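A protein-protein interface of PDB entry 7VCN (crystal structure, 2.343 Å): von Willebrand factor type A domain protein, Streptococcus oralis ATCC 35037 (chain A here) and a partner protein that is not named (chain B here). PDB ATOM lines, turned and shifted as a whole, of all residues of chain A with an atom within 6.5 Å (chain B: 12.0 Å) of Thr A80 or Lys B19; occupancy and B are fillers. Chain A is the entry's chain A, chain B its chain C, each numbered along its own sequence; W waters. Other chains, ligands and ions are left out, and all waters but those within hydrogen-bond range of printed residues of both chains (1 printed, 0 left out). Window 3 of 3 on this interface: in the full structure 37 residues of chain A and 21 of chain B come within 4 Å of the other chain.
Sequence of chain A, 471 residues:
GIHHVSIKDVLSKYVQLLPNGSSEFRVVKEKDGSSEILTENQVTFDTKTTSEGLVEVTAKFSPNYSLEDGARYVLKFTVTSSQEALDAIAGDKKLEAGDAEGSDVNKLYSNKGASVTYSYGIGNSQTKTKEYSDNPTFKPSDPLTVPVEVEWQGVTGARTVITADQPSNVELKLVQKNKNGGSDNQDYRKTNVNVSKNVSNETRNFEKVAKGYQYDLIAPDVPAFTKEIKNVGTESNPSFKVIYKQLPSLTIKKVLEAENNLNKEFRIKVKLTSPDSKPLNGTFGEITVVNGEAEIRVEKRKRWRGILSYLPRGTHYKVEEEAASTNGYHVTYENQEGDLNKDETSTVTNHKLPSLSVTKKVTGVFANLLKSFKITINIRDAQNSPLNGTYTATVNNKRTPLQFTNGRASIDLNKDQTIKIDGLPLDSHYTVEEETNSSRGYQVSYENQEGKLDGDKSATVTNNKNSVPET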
ATOM      1  N   TYR A  14      -0.207 -29.441 -10.123  1.00  0.00           N
ATOM      2  CA  TYR A  14       0.733 -29.398 -11.232  1.00  0.00           C
ATOM      3  C   TYR A  14       0.129 -28.814 -12.511  1.00  0.00           C
ATOM      4  O   TYR A  14       0.869 -28.558 -13.457  1.00  0.00           O
ATOM      5  CB  TYR A  14       1.279 -30.805 -11.464  1.00  0.00           C
ATOM      6  CG  TYR A  14       2.193 -31.221 -10.347  1.00  0.00           C
ATOM      7  CD1 TYR A  14       3.444 -30.623 -10.220  1.00  0.00           C
ATOM      8  CD2 TYR A  14       1.793 -32.096  -9.351  1.00  0.00           C
ATOM      9  CE1 TYR A  14       4.296 -30.936  -9.174  1.00  0.00           C
ATOM     10  CE2 TYR A  14       2.642 -32.413  -8.296  1.00  0.00           C
ATOM     11  CZ  TYR A  14       3.895 -31.814  -8.193  1.00  0.00           C
ATOM     12  OH  TYR A  14       4.763 -32.113  -7.175  1.00  0.00           O
ATOM     13  N   VAL A  15      -1.199 -28.607 -12.563  1.00  0.00           N
ATOM     14  CA  VAL A  15      -1.741 -27.902 -13.724  1.00  0.00           C
ATOM     15  C   VAL A  15      -2.673 -26.819 -13.226  1.00  0.00           C
ATOM     16  O   VAL A  15      -3.001 -26.845 -12.040  1.00  0.00           O
ATOM     17  CB  VAL A  15      -2.531 -28.817 -14.657  1.00  0.00           C
ATOM     18  CG1 VAL A  15      -1.678 -29.981 -15.133  1.00  0.00           C
ATOM     19  CG2 VAL A  15      -3.808 -29.277 -13.970  1.00  0.00           C
ATOM     20  N   GLN A  16      -3.165 -26.012 -14.173  1.00  0.00           N
ATOM     21  CA  GLN A  16      -4.086 -24.928 -13.909  1.00  0.00           C
ATOM     22  C   GLN A  16      -4.760 -24.468 -15.213  1.00  0.00           C
ATOM     23  O   GLN A  16      -4.327 -24.803 -16.305  1.00  0.00           O
ATOM     24  CB  GLN A  16      -3.325 -23.822 -13.196  1.00  0.00           C
ATOM     25  CG  GLN A  16      -2.539 -22.962 -14.138  1.00  0.00           C
ATOM     26  CD  GLN A  16      -1.505 -22.049 -13.547  1.00  0.00           C
ATOM     27  OE1 GLN A  16      -0.889 -22.313 -12.505  1.00  0.00           O
ATOM     28  NE2 GLN A  16      -1.275 -20.976 -14.266  1.00  0.00           N
ATOM     29  N   LEU A  17      -5.866 -23.727 -15.067  1.00  0.00           N
ATOM     30  CA  LEU A  17      -6.713 -23.300 -16.163  1.00  0.00           C
ATOM     31  C   LEU A  17      -5.980 -22.159 -16.821  1.00  0.00           C
ATOM     32  O   LEU A  17      -4.958 -21.745 -16.292  1.00  0.00           O
ATOM     33  CB  LEU A  17      -8.057 -22.830 -15.597  1.00  0.00           C
ATOM     34  CG  LEU A  17      -8.881 -23.923 -14.921  1.00  0.00           C
ATOM     35  CD1 LEU A  17     -10.217 -23.376 -14.525  1.00  0.00           C
ATOM     36  CD2 LEU A  17      -9.074 -25.127 -15.832  1.00  0.00           C
ATOM     37  N   LEU A  18      -6.464 -21.705 -17.981  1.00  0.00           N
ATOM     38  CA  LEU A  18      -5.859 -20.596 -18.687  1.00  0.00           C
ATOM     39  C   LEU A  18      -6.553 -19.319 -18.241  1.00  0.00           C
ATOM     40  O   LEU A  18      -7.698 -19.400 -17.819  1.00  0.00           O
ATOM     41  CB  LEU A  18      -6.061 -20.855 -20.180  1.00  0.00           C
ATOM     42  CG  LEU A  18      -5.241 -22.019 -20.751  1.00  0.00           C
ATOM     43  CD1 LEU A  18      -5.491 -22.194 -22.247  1.00  0.00           C
ATOM     44  CD2 LEU A  18      -3.753 -21.827 -20.509  1.00  0.00           C
ATOM     45  N   PRO A  19      -5.938 -18.113 -18.384  1.00  0.00           N
ATOM     46  CA  PRO A  19      -6.633 -16.843 -18.073  1.00  0.00           C
ATOM     47  C   PRO A  19      -7.934 -16.666 -18.868  1.00  0.00           C
ATOM     48  O   PRO A  19      -8.016 -17.157 -20.000  1.00  0.00           O
ATOM     49  CB  PRO A  19      -5.680 -15.759 -18.586  1.00  0.00           C
ATOM     50  CG  PRO A  19      -4.590 -16.486 -19.404  1.00  0.00           C
ATOM     51  CD  PRO A  19      -4.594 -17.929 -18.975  1.00  0.00           C
ATOM     52  N   SER A  23      -9.381 -21.553 -21.522  1.00  0.00           N
ATOM     53  CA  SER A  23      -9.543 -22.985 -21.274  1.00  0.00           C
ATOM     54  C   SER A  23     -10.668 -23.617 -22.120  1.00  0.00           C
ATOM     55  O   SER A  23     -10.580 -24.812 -22.412  1.00  0.00           O
ATOM     56  CB  SER A  23      -9.704 -23.260 -19.805  1.00  0.00           C
ATOM     57  OG  SER A  23      -8.440 -23.445 -19.212  1.00  0.00           O
ATOM     58  N   THR A  78      -8.686 -27.002 -21.737  1.00  0.00           N
ATOM     59  CA  THR A  78      -7.227 -27.027 -21.759  1.00  0.00           C
ATOM     60  C   THR A  78      -6.710 -26.688 -20.355  1.00  0.00           C
ATOM     61  O   THR A  78      -7.245 -25.817 -19.676  1.00  0.00           O
ATOM     62  CB  THR A  78      -6.751 -25.964 -22.741  1.00  0.00           C
ATOM     63  OG1 THR A  78      -7.308 -26.260 -24.023  1.00  0.00           O
ATOM     64  CG2 THR A  78      -5.250 -25.793 -22.803  1.00  0.00           C
ATOM     65  N   VAL A  79      -5.676 -27.390 -19.903  1.00  0.00           N
ATOM     66  CA  VAL A  79      -4.884 -26.877 -18.791  1.00  0.00           C
ATOM     67  C   VAL A  79      -3.457 -26.568 -19.222  1.00  0.00           C
ATOM     68  O   VAL A  79      -3.009 -27.058 -20.253  1.00  0.00           O
ATOM     69  CB  VAL A  79      -4.906 -27.852 -17.633  1.00  0.00           C
ATOM     70  CG1 VAL A  79      -6.348 -27.928 -17.120  1.00  0.00           C
ATOM     71  CG2 VAL A  79      -4.351 -29.192 -18.074  1.00  0.00           C
ATOM     72  N   THR A  80      -2.747 -25.777 -18.400  1.00  0.00           N
ATOM     73  CA  THR A  80      -1.335 -25.534 -18.631  1.00  0.00           C
ATOM     74  C   THR A  80      -0.542 -25.987 -17.414  1.00  0.00           C
ATOM     75  O   THR A  80      -1.082 -26.005 -16.325  1.00  0.00           O
ATOM     76  CB  THR A  80      -1.125 -24.046 -18.913  1.00  0.00           C
ATOM     77  OG1 THR A  80       0.282 -23.840 -19.031  1.00  0.00           O
ATOM     78  CG2 THR A  80      -1.587 -23.135 -17.791  1.00  0.00           C
ATOM     79  N   SER A  81       0.736 -26.342 -17.598  1.00  0.00           N
ATOM     80  CA  SER A  81       1.645 -26.633 -16.486  1.00  0.00           C
ATOM     81  C   SER A  81       1.653 -25.467 -15.502  1.00  0.00           C
ATOM     82  O   SER A  81       1.906 -24.344 -15.927  1.00  0.00           O
ATOM     83  CB  SER A  81       3.076 -26.805 -17.003  1.00  0.00           C
ATOM     84  OG  SER A  81       3.130 -27.821 -18.015  1.00  0.00           O
ATOM     85  N   SER A  82       1.476 -25.741 -14.202  1.00  0.00           N
ATOM     86  CA  SER A  82       1.624 -24.706 -13.165  1.00  0.00           C
ATOM     87  C   SER A  82       3.118 -24.469 -12.911  1.00  0.00           C
ATOM     88  O   SER A  82       3.942 -25.260 -13.348  1.00  0.00           O
ATOM     89  CB  SER A  82       0.964 -25.166 -11.880  1.00  0.00           C
ATOM     90  OG  SER A  82       1.739 -26.201 -11.303  1.00  0.00           O
ATOM     91  N   PHE A 138       1.237 -36.414 -17.476  1.00  0.00           N
ATOM     92  CA  PHE A 138       1.841 -35.608 -18.525  1.00  0.00           C
ATOM     93  C   PHE A 138       3.248 -35.220 -18.117  1.00  0.00           C
ATOM     94  O   PHE A 138       3.600 -35.257 -16.932  1.00  0.00           O
ATOM     95  CB  PHE A 138       1.026 -34.336 -18.675  1.00  0.00           C
ATOM     96  CG  PHE A 138       1.139 -33.356 -17.526  1.00  0.00           C
ATOM     97  CD1 PHE A 138       0.340 -33.491 -16.386  1.00  0.00           C
ATOM     98  CD2 PHE A 138       2.007 -32.253 -17.592  1.00  0.00           C
ATOM     99  CE1 PHE A 138       0.431 -32.565 -15.348  1.00  0.00           C
ATOM    100  CE2 PHE A 138       2.133 -31.364 -16.526  1.00  0.00           C
ATOM    101  CZ  PHE A 138       1.342 -31.507 -15.410  1.00  0.00           C
ATOM    102  N   THR B   9      -8.931 -38.888 -20.532  1.00  0.00           N
ATOM    103  CA  THR B   9      -7.554 -38.846 -21.067  1.00  0.00           C
ATOM    104  C   THR B   9      -6.995 -37.423 -20.973  1.00  0.00           C
ATOM    105  O   THR B   9      -7.785 -36.467 -20.873  1.00  0.00           O
ATOM    106  CB  THR B   9      -7.526 -39.199 -22.574  1.00  0.00           C
ATOM    107  OG1 THR B   9      -7.951 -38.048 -23.305  1.00  0.00           O
ATOM    108  CG2 THR B   9      -8.435 -40.324 -23.012  1.00  0.00           C
ATOM    109  N   ILE B  10      -5.673 -37.246 -21.082  1.00  0.00           N
ATOM    110  CA  ILE B  10      -5.080 -35.913 -21.303  1.00  0.00           C
ATOM    111  C   ILE B  10      -4.262 -35.976 -22.596  1.00  0.00           C
ATOM    112  O   ILE B  10      -3.626 -36.973 -22.886  1.00  0.00           O
ATOM    113  CB  ILE B  10      -4.211 -35.474 -20.104  1.00  0.00           C
ATOM    114  CG1 ILE B  10      -3.790 -34.009 -20.182  1.00  0.00           C
ATOM    115  CG2 ILE B  10      -3.004 -36.367 -19.907  1.00  0.00           C
ATOM    116  CD1 ILE B  10      -3.130 -33.440 -18.904  1.00  0.00           C
ATOM    117  N   THR B  11      -4.235 -34.931 -23.414  1.00  0.00           N
ATOM    118  CA  THR B  11      -3.446 -35.016 -24.643  1.00  0.00           C
ATOM    119  C   THR B  11      -2.563 -33.784 -24.762  1.00  0.00           C
ATOM    120  O   THR B  11      -3.085 -32.686 -24.677  1.00  0.00           O
ATOM    121  CB  THR B  11      -4.396 -35.036 -25.852  1.00  0.00           C
ATOM    122  OG1 THR B  11      -5.166 -36.219 -25.655  1.00  0.00           O
ATOM    123  CG2 THR B  11      -3.744 -35.127 -27.209  1.00  0.00           C
ATOM    124  N   PRO B  12      -1.226 -33.882 -24.986  1.00  0.00           N
ATOM    125  CA  PRO B  12      -0.405 -32.687 -25.277  1.00  0.00           C
ATOM    126  C   PRO B  12      -1.010 -31.977 -26.483  1.00  0.00           C
ATOM    127  O   PRO B  12      -1.488 -32.646 -27.387  1.00  0.00           O
ATOM    128  CB  PRO B  12       0.939 -33.304 -25.629  1.00  0.00           C
ATOM    129  CG  PRO B  12       0.960 -34.459 -24.710  1.00  0.00           C
ATOM    130  CD  PRO B  12      -0.408 -35.102 -24.933  1.00  0.00           C
ATOM    131  N   ILE B  13      -1.114 -30.644 -26.415  1.00  0.00           N
ATOM    132  CA  ILE B  13      -1.639 -29.891 -27.544  1.00  0.00           C
ATOM    133  C   ILE B  13      -0.497 -29.648 -28.509  1.00  0.00           C
ATOM    134  O   ILE B  13       0.444 -28.955 -28.145  1.00  0.00           O
ATOM    135  CB  ILE B  13      -2.329 -28.574 -27.149  1.00  0.00           C
ATOM    136  CG1 ILE B  13      -3.672 -28.856 -26.476  1.00  0.00           C
ATOM    137  CG2 ILE B  13      -2.454 -27.697 -28.388  1.00  0.00           C
ATOM    138  CD1 ILE B  13      -4.438 -27.626 -26.200  1.00  0.00           C
ATOM    139  N   SER B  14      -0.605 -30.257 -29.693  1.00  0.00           N
ATOM    140  CA  SER B  14       0.447 -30.256 -30.701  1.00  0.00           C
ATOM    141  C   SER B  14       1.012 -28.855 -30.898  1.00  0.00           C
ATOM    142  O   SER B  14       0.251 -27.903 -31.063  1.00  0.00           O
ATOM    143  CB  SER B  14      -0.065 -30.801 -32.002  1.00  0.00           C
ATOM    144  OG  SER B  14       1.008 -31.315 -32.790  1.00  0.00           O
ATOM    145  N   GLY B  15       2.339 -28.757 -30.835  1.00  0.00           N
ATOM    146  CA  GLY B  15       3.069 -27.575 -31.250  1.00  0.00           C
ATOM    147  C   GLY B  15       3.104 -26.472 -30.195  1.00  0.00           C
ATOM    148  O   GLY B  15       3.606 -25.410 -30.481  1.00  0.00           O
ATOM    149  N   GLN B  16       2.547 -26.736 -29.005  1.00  0.00           N
ATOM    150  CA  GLN B  16       2.490 -25.772 -27.927  1.00  0.00           C
ATOM    151  C   GLN B  16       3.168 -26.330 -26.686  1.00  0.00           C
ATOM    152  O   GLN B  16       2.912 -27.464 -26.325  1.00  0.00           O
ATOM    153  CB  GLN B  16       1.051 -25.359 -27.645  1.00  0.00           C
ATOM    154  CG  GLN B  16       0.562 -24.232 -28.540  1.00  0.00           C
ATOM    155  CD  GLN B  16      -0.944 -24.142 -28.459  1.00  0.00           C
ATOM    156  OE1 GLN B  16      -1.486 -24.005 -27.378  1.00  0.00           O
ATOM    157  NE2 GLN B  16      -1.634 -24.213 -29.591  1.00  0.00           N
ATOM    158  N   ASP B  17       3.996 -25.510 -26.048  1.00  0.00           N
ATOM    159  CA  ASP B  17       4.758 -25.870 -24.844  1.00  0.00           C
ATOM    160  C   ASP B  17       3.811 -25.756 -23.665  1.00  0.00           C
ATOM    161  O   ASP B  17       3.182 -24.733 -23.549  1.00  0.00           O
ATOM    162  CB  ASP B  17       5.978 -24.929 -24.630  1.00  0.00           C
ATOM    163  CG  ASP B  17       7.325 -25.243 -25.191  1.00  0.00           C
ATOM    164  OD1 ASP B  17       8.045 -26.001 -24.519  1.00  0.00           O
ATOM    165  OD2 ASP B  17       7.535 -24.812 -26.318  1.00  0.00           O
ATOM    166  N   ASP B  18       3.714 -26.793 -22.852  1.00  0.00           N
ATOM    167  CA  ASP B  18       2.988 -26.770 -21.583  1.00  0.00           C
ATOM    168  C   ASP B  18       1.458 -26.647 -21.714  1.00  0.00           C
ATOM    169  O   ASP B  18       0.839 -26.210 -20.746  1.00  0.00           O
ATOM    170  CB  ASP B  18       3.548 -25.747 -20.600  1.00  0.00           C
ATOM    171  CG  ASP B  18       5.008 -26.004 -20.257  1.00  0.00           C
ATOM    172  OD1 ASP B  18       5.303 -27.081 -19.694  1.00  0.00           O
ATOM    173  OD2 ASP B  18       5.848 -25.121 -20.590  1.00  0.00           O
ATOM    174  N   LYS B  19       0.846 -27.017 -22.862  1.00  0.00           N
ATOM    175  CA  LYS B  19      -0.599 -26.991 -22.894  1.00  0.00           C
ATOM    176  C   LYS B  19      -1.129 -28.398 -23.175  1.00  0.00           C
ATOM    177  O   LYS B  19      -0.543 -29.114 -23.964  1.00  0.00           O
ATOM    178  CB  LYS B  19      -1.059 -25.997 -23.942  1.00  0.00           C
ATOM    179  CG  LYS B  19      -0.430 -24.622 -23.866  1.00  0.00           C
ATOM    180  CD  LYS B  19      -1.487 -23.507 -24.032  1.00  0.00           C
ATOM    181  CE  LYS B  19      -0.971 -22.119 -23.703  1.00  0.00           C
ATOM    182  NZ  LYS B  19      -0.125 -22.186 -22.481  1.00  0.00           N
ATOM    183  N   TYR B  20      -2.235 -28.796 -22.531  1.00  0.00           N
ATOM    184  CA  TYR B  20      -2.764 -30.156 -22.622  1.00  0.00           C
ATOM    185  C   TYR B  20      -4.282 -30.074 -22.619  1.00  0.00           C
ATOM    186  O   TYR B  20      -4.858 -29.191 -21.985  1.00  0.00           O
ATOM    187  CB  TYR B  20      -2.343 -30.979 -21.388  1.00  0.00           C
ATOM    188  CG  TYR B  20      -0.872 -30.853 -21.076  1.00  0.00           C
ATOM    189  CD1 TYR B  20      -0.383 -29.730 -20.426  1.00  0.00           C
ATOM    190  CD2 TYR B  20       0.039 -31.780 -21.556  1.00  0.00           C
ATOM    191  CE1 TYR B  20       0.988 -29.543 -20.223  1.00  0.00           C
ATOM    192  CE2 TYR B  20       1.398 -31.633 -21.339  1.00  0.00           C
ATOM    193  CZ  TYR B  20       1.876 -30.520 -20.659  1.00  0.00           C
ATOM    194  OH  TYR B  20       3.218 -30.375 -20.420  1.00  0.00           O
ATOM    195  N   GLU B  21      -4.934 -30.970 -23.349  1.00  0.00           N
ATOM    196  CA  GLU B  21      -6.388 -30.976 -23.386  1.00  0.00           C
ATOM    197  C   GLU B  21      -6.878 -32.109 -22.521  1.00  0.00           C
ATOM    198  O   GLU B  21      -6.395 -33.228 -22.719  1.00  0.00           O
ATOM    199  CB  GLU B  21      -6.886 -31.165 -24.818  1.00  0.00           C
ATOM    200  CG  GLU B  21      -8.397 -31.340 -24.870  1.00  0.00           C
ATOM    201  CD  GLU B  21      -8.989 -30.863 -26.196  1.00  0.00           C
ATOM    202  OE1 GLU B  21      -9.124 -29.621 -26.415  1.00  0.00           O
ATOM    203  OE2 GLU B  21      -9.371 -31.724 -27.022  1.00  0.00           O
ATOM    204  N   LEU B  22      -7.739 -31.809 -21.534  1.00  0.00           N
ATOM    205  CA  LEU B  22      -8.338 -32.860 -20.726  1.00  0.00           C
ATOM    206  C   LEU B  22      -9.622 -33.307 -21.390  1.00  0.00           C
ATOM    207  O   LEU B  22     -10.349 -32.505 -22.004  1.00  0.00           O
ATOM    208  CB  LEU B  22      -8.594 -32.383 -19.308  1.00  0.00           C
ATOM    209  CG  LEU B  22      -7.392 -32.626 -18.387  1.00  0.00           C
ATOM    210  CD1 LEU B  22      -7.304 -31.670 -17.199  1.00  0.00           C
ATOM    211  CD2 LEU B  22      -7.318 -34.070 -17.927  1.00  0.00           C
ATOM    212  N   SER B  23      -9.941 -34.588 -21.249  1.00  0.00           N
ATOM    213  CA  SER B  23     -11.168 -35.060 -21.877  1.00  0.00           C
ATOM    214  C   SER B  23     -11.853 -36.027 -20.920  1.00  0.00           C
ATOM    215  O   SER B  23     -11.300 -37.083 -20.611  1.00  0.00           O
ATOM    216  CB  SER B  23     -10.824 -35.689 -23.221  1.00  0.00           C
ATOM    217  OG  SER B  23     -11.934 -36.483 -23.654  1.00  0.00           O
HETATM  218  O   HOH W   1      -9.975 -27.461 -24.872  1.00  0.00           O
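The side-chain hydroxyl of Thr A80 is in hydrogen-bond range of the backbone carbonyl oxygen of Asp B18 (3.0 Å). The side-chain hydroxyl (OG) of Ser A81 lies within hydrogen-bond range of the side-chain carboxylate (OD1) of Asp B18, at 2.8 Å. The backbone NH (N) of Val A79 is in hydrogen-bond range of the backbone carbonyl oxygen (O) of Tyr B20, 2.9 Å away.
N of Ile B13 lies within hydrogen-bond range of O of Lys B19 (2.9 Å). N of Thr A80 sits at hydrogen-bond distance from O of Gln A16. O of Thr A78 lies within hydrogen-bond range of OG of Ser A23 (2.7 Å).
Among the printed residues, merely in contact across the chains: Thr A78 with Ile B13, Thr A78 with Tyr B20, Val A79 with Asp B18, Val A79 with Lys B19, Val A79 with Leu B22, Thr A80 with Lys B19, Ser A81 with Tyr B20 and Phe A138 with Tyr B20.
Of chain B, only Asp B18 (3.0 Å) and Lys B19 (3.8 Å) come within 4 Å of Thr A80. Of chain A, only Val A79 (3.6 Å) and Thr A80 (3.8 Å) come within 4 Å of Lys B19. No residue of chain B comes within 4 Å of Gln A16. No residue of chain B comes within 4 Å of Leu A18. Of chain B, only Asp B18 (2.8 Å) and Tyr B20 (3.5 Å) come within 4 Å of Ser A81. No residue of chain B comes within 4 Å of Ser A82. Of the printed residues of chain A, Ile B13 touches Thr A78. Printed residues of chain A within 4 Å of Asp B18: Val A79 (3.97 Å), Thr A80 (3.0 Å) and Ser A81 (2.8 Å). Of the printed residues of chain A, Tyr B20 touches Thr A78, Val A79, Ser A81 and Phe A138. Printed residues of chain A within 4 Å of Leu B22: Val A79. Ser A23 touches none of the printed residues of chain B. The nearest residue of chain A that does not touch Lys B19 is Leu A18 (4.1 Å).
Of the 15 printed residues of chain B, 5 touch a printed residue of chain A. Hydrophobic or aromatic side chains of chain B within 4 Å of the printed part of chain A: Ile B13, Tyr B20 and Leu B22. Along chain B the printed residues that touch a printed residue of chain A span positions 13 to 22. Among the printed residues, no Asp or Glu carboxylate lies within 4 Å of a Lys or Arg side-chain nitrogen of the other chain.
Water W1 bridges OE1 of Glu B21 (2.8 Å) and OG1 of Thr A78 (3.0 Å).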
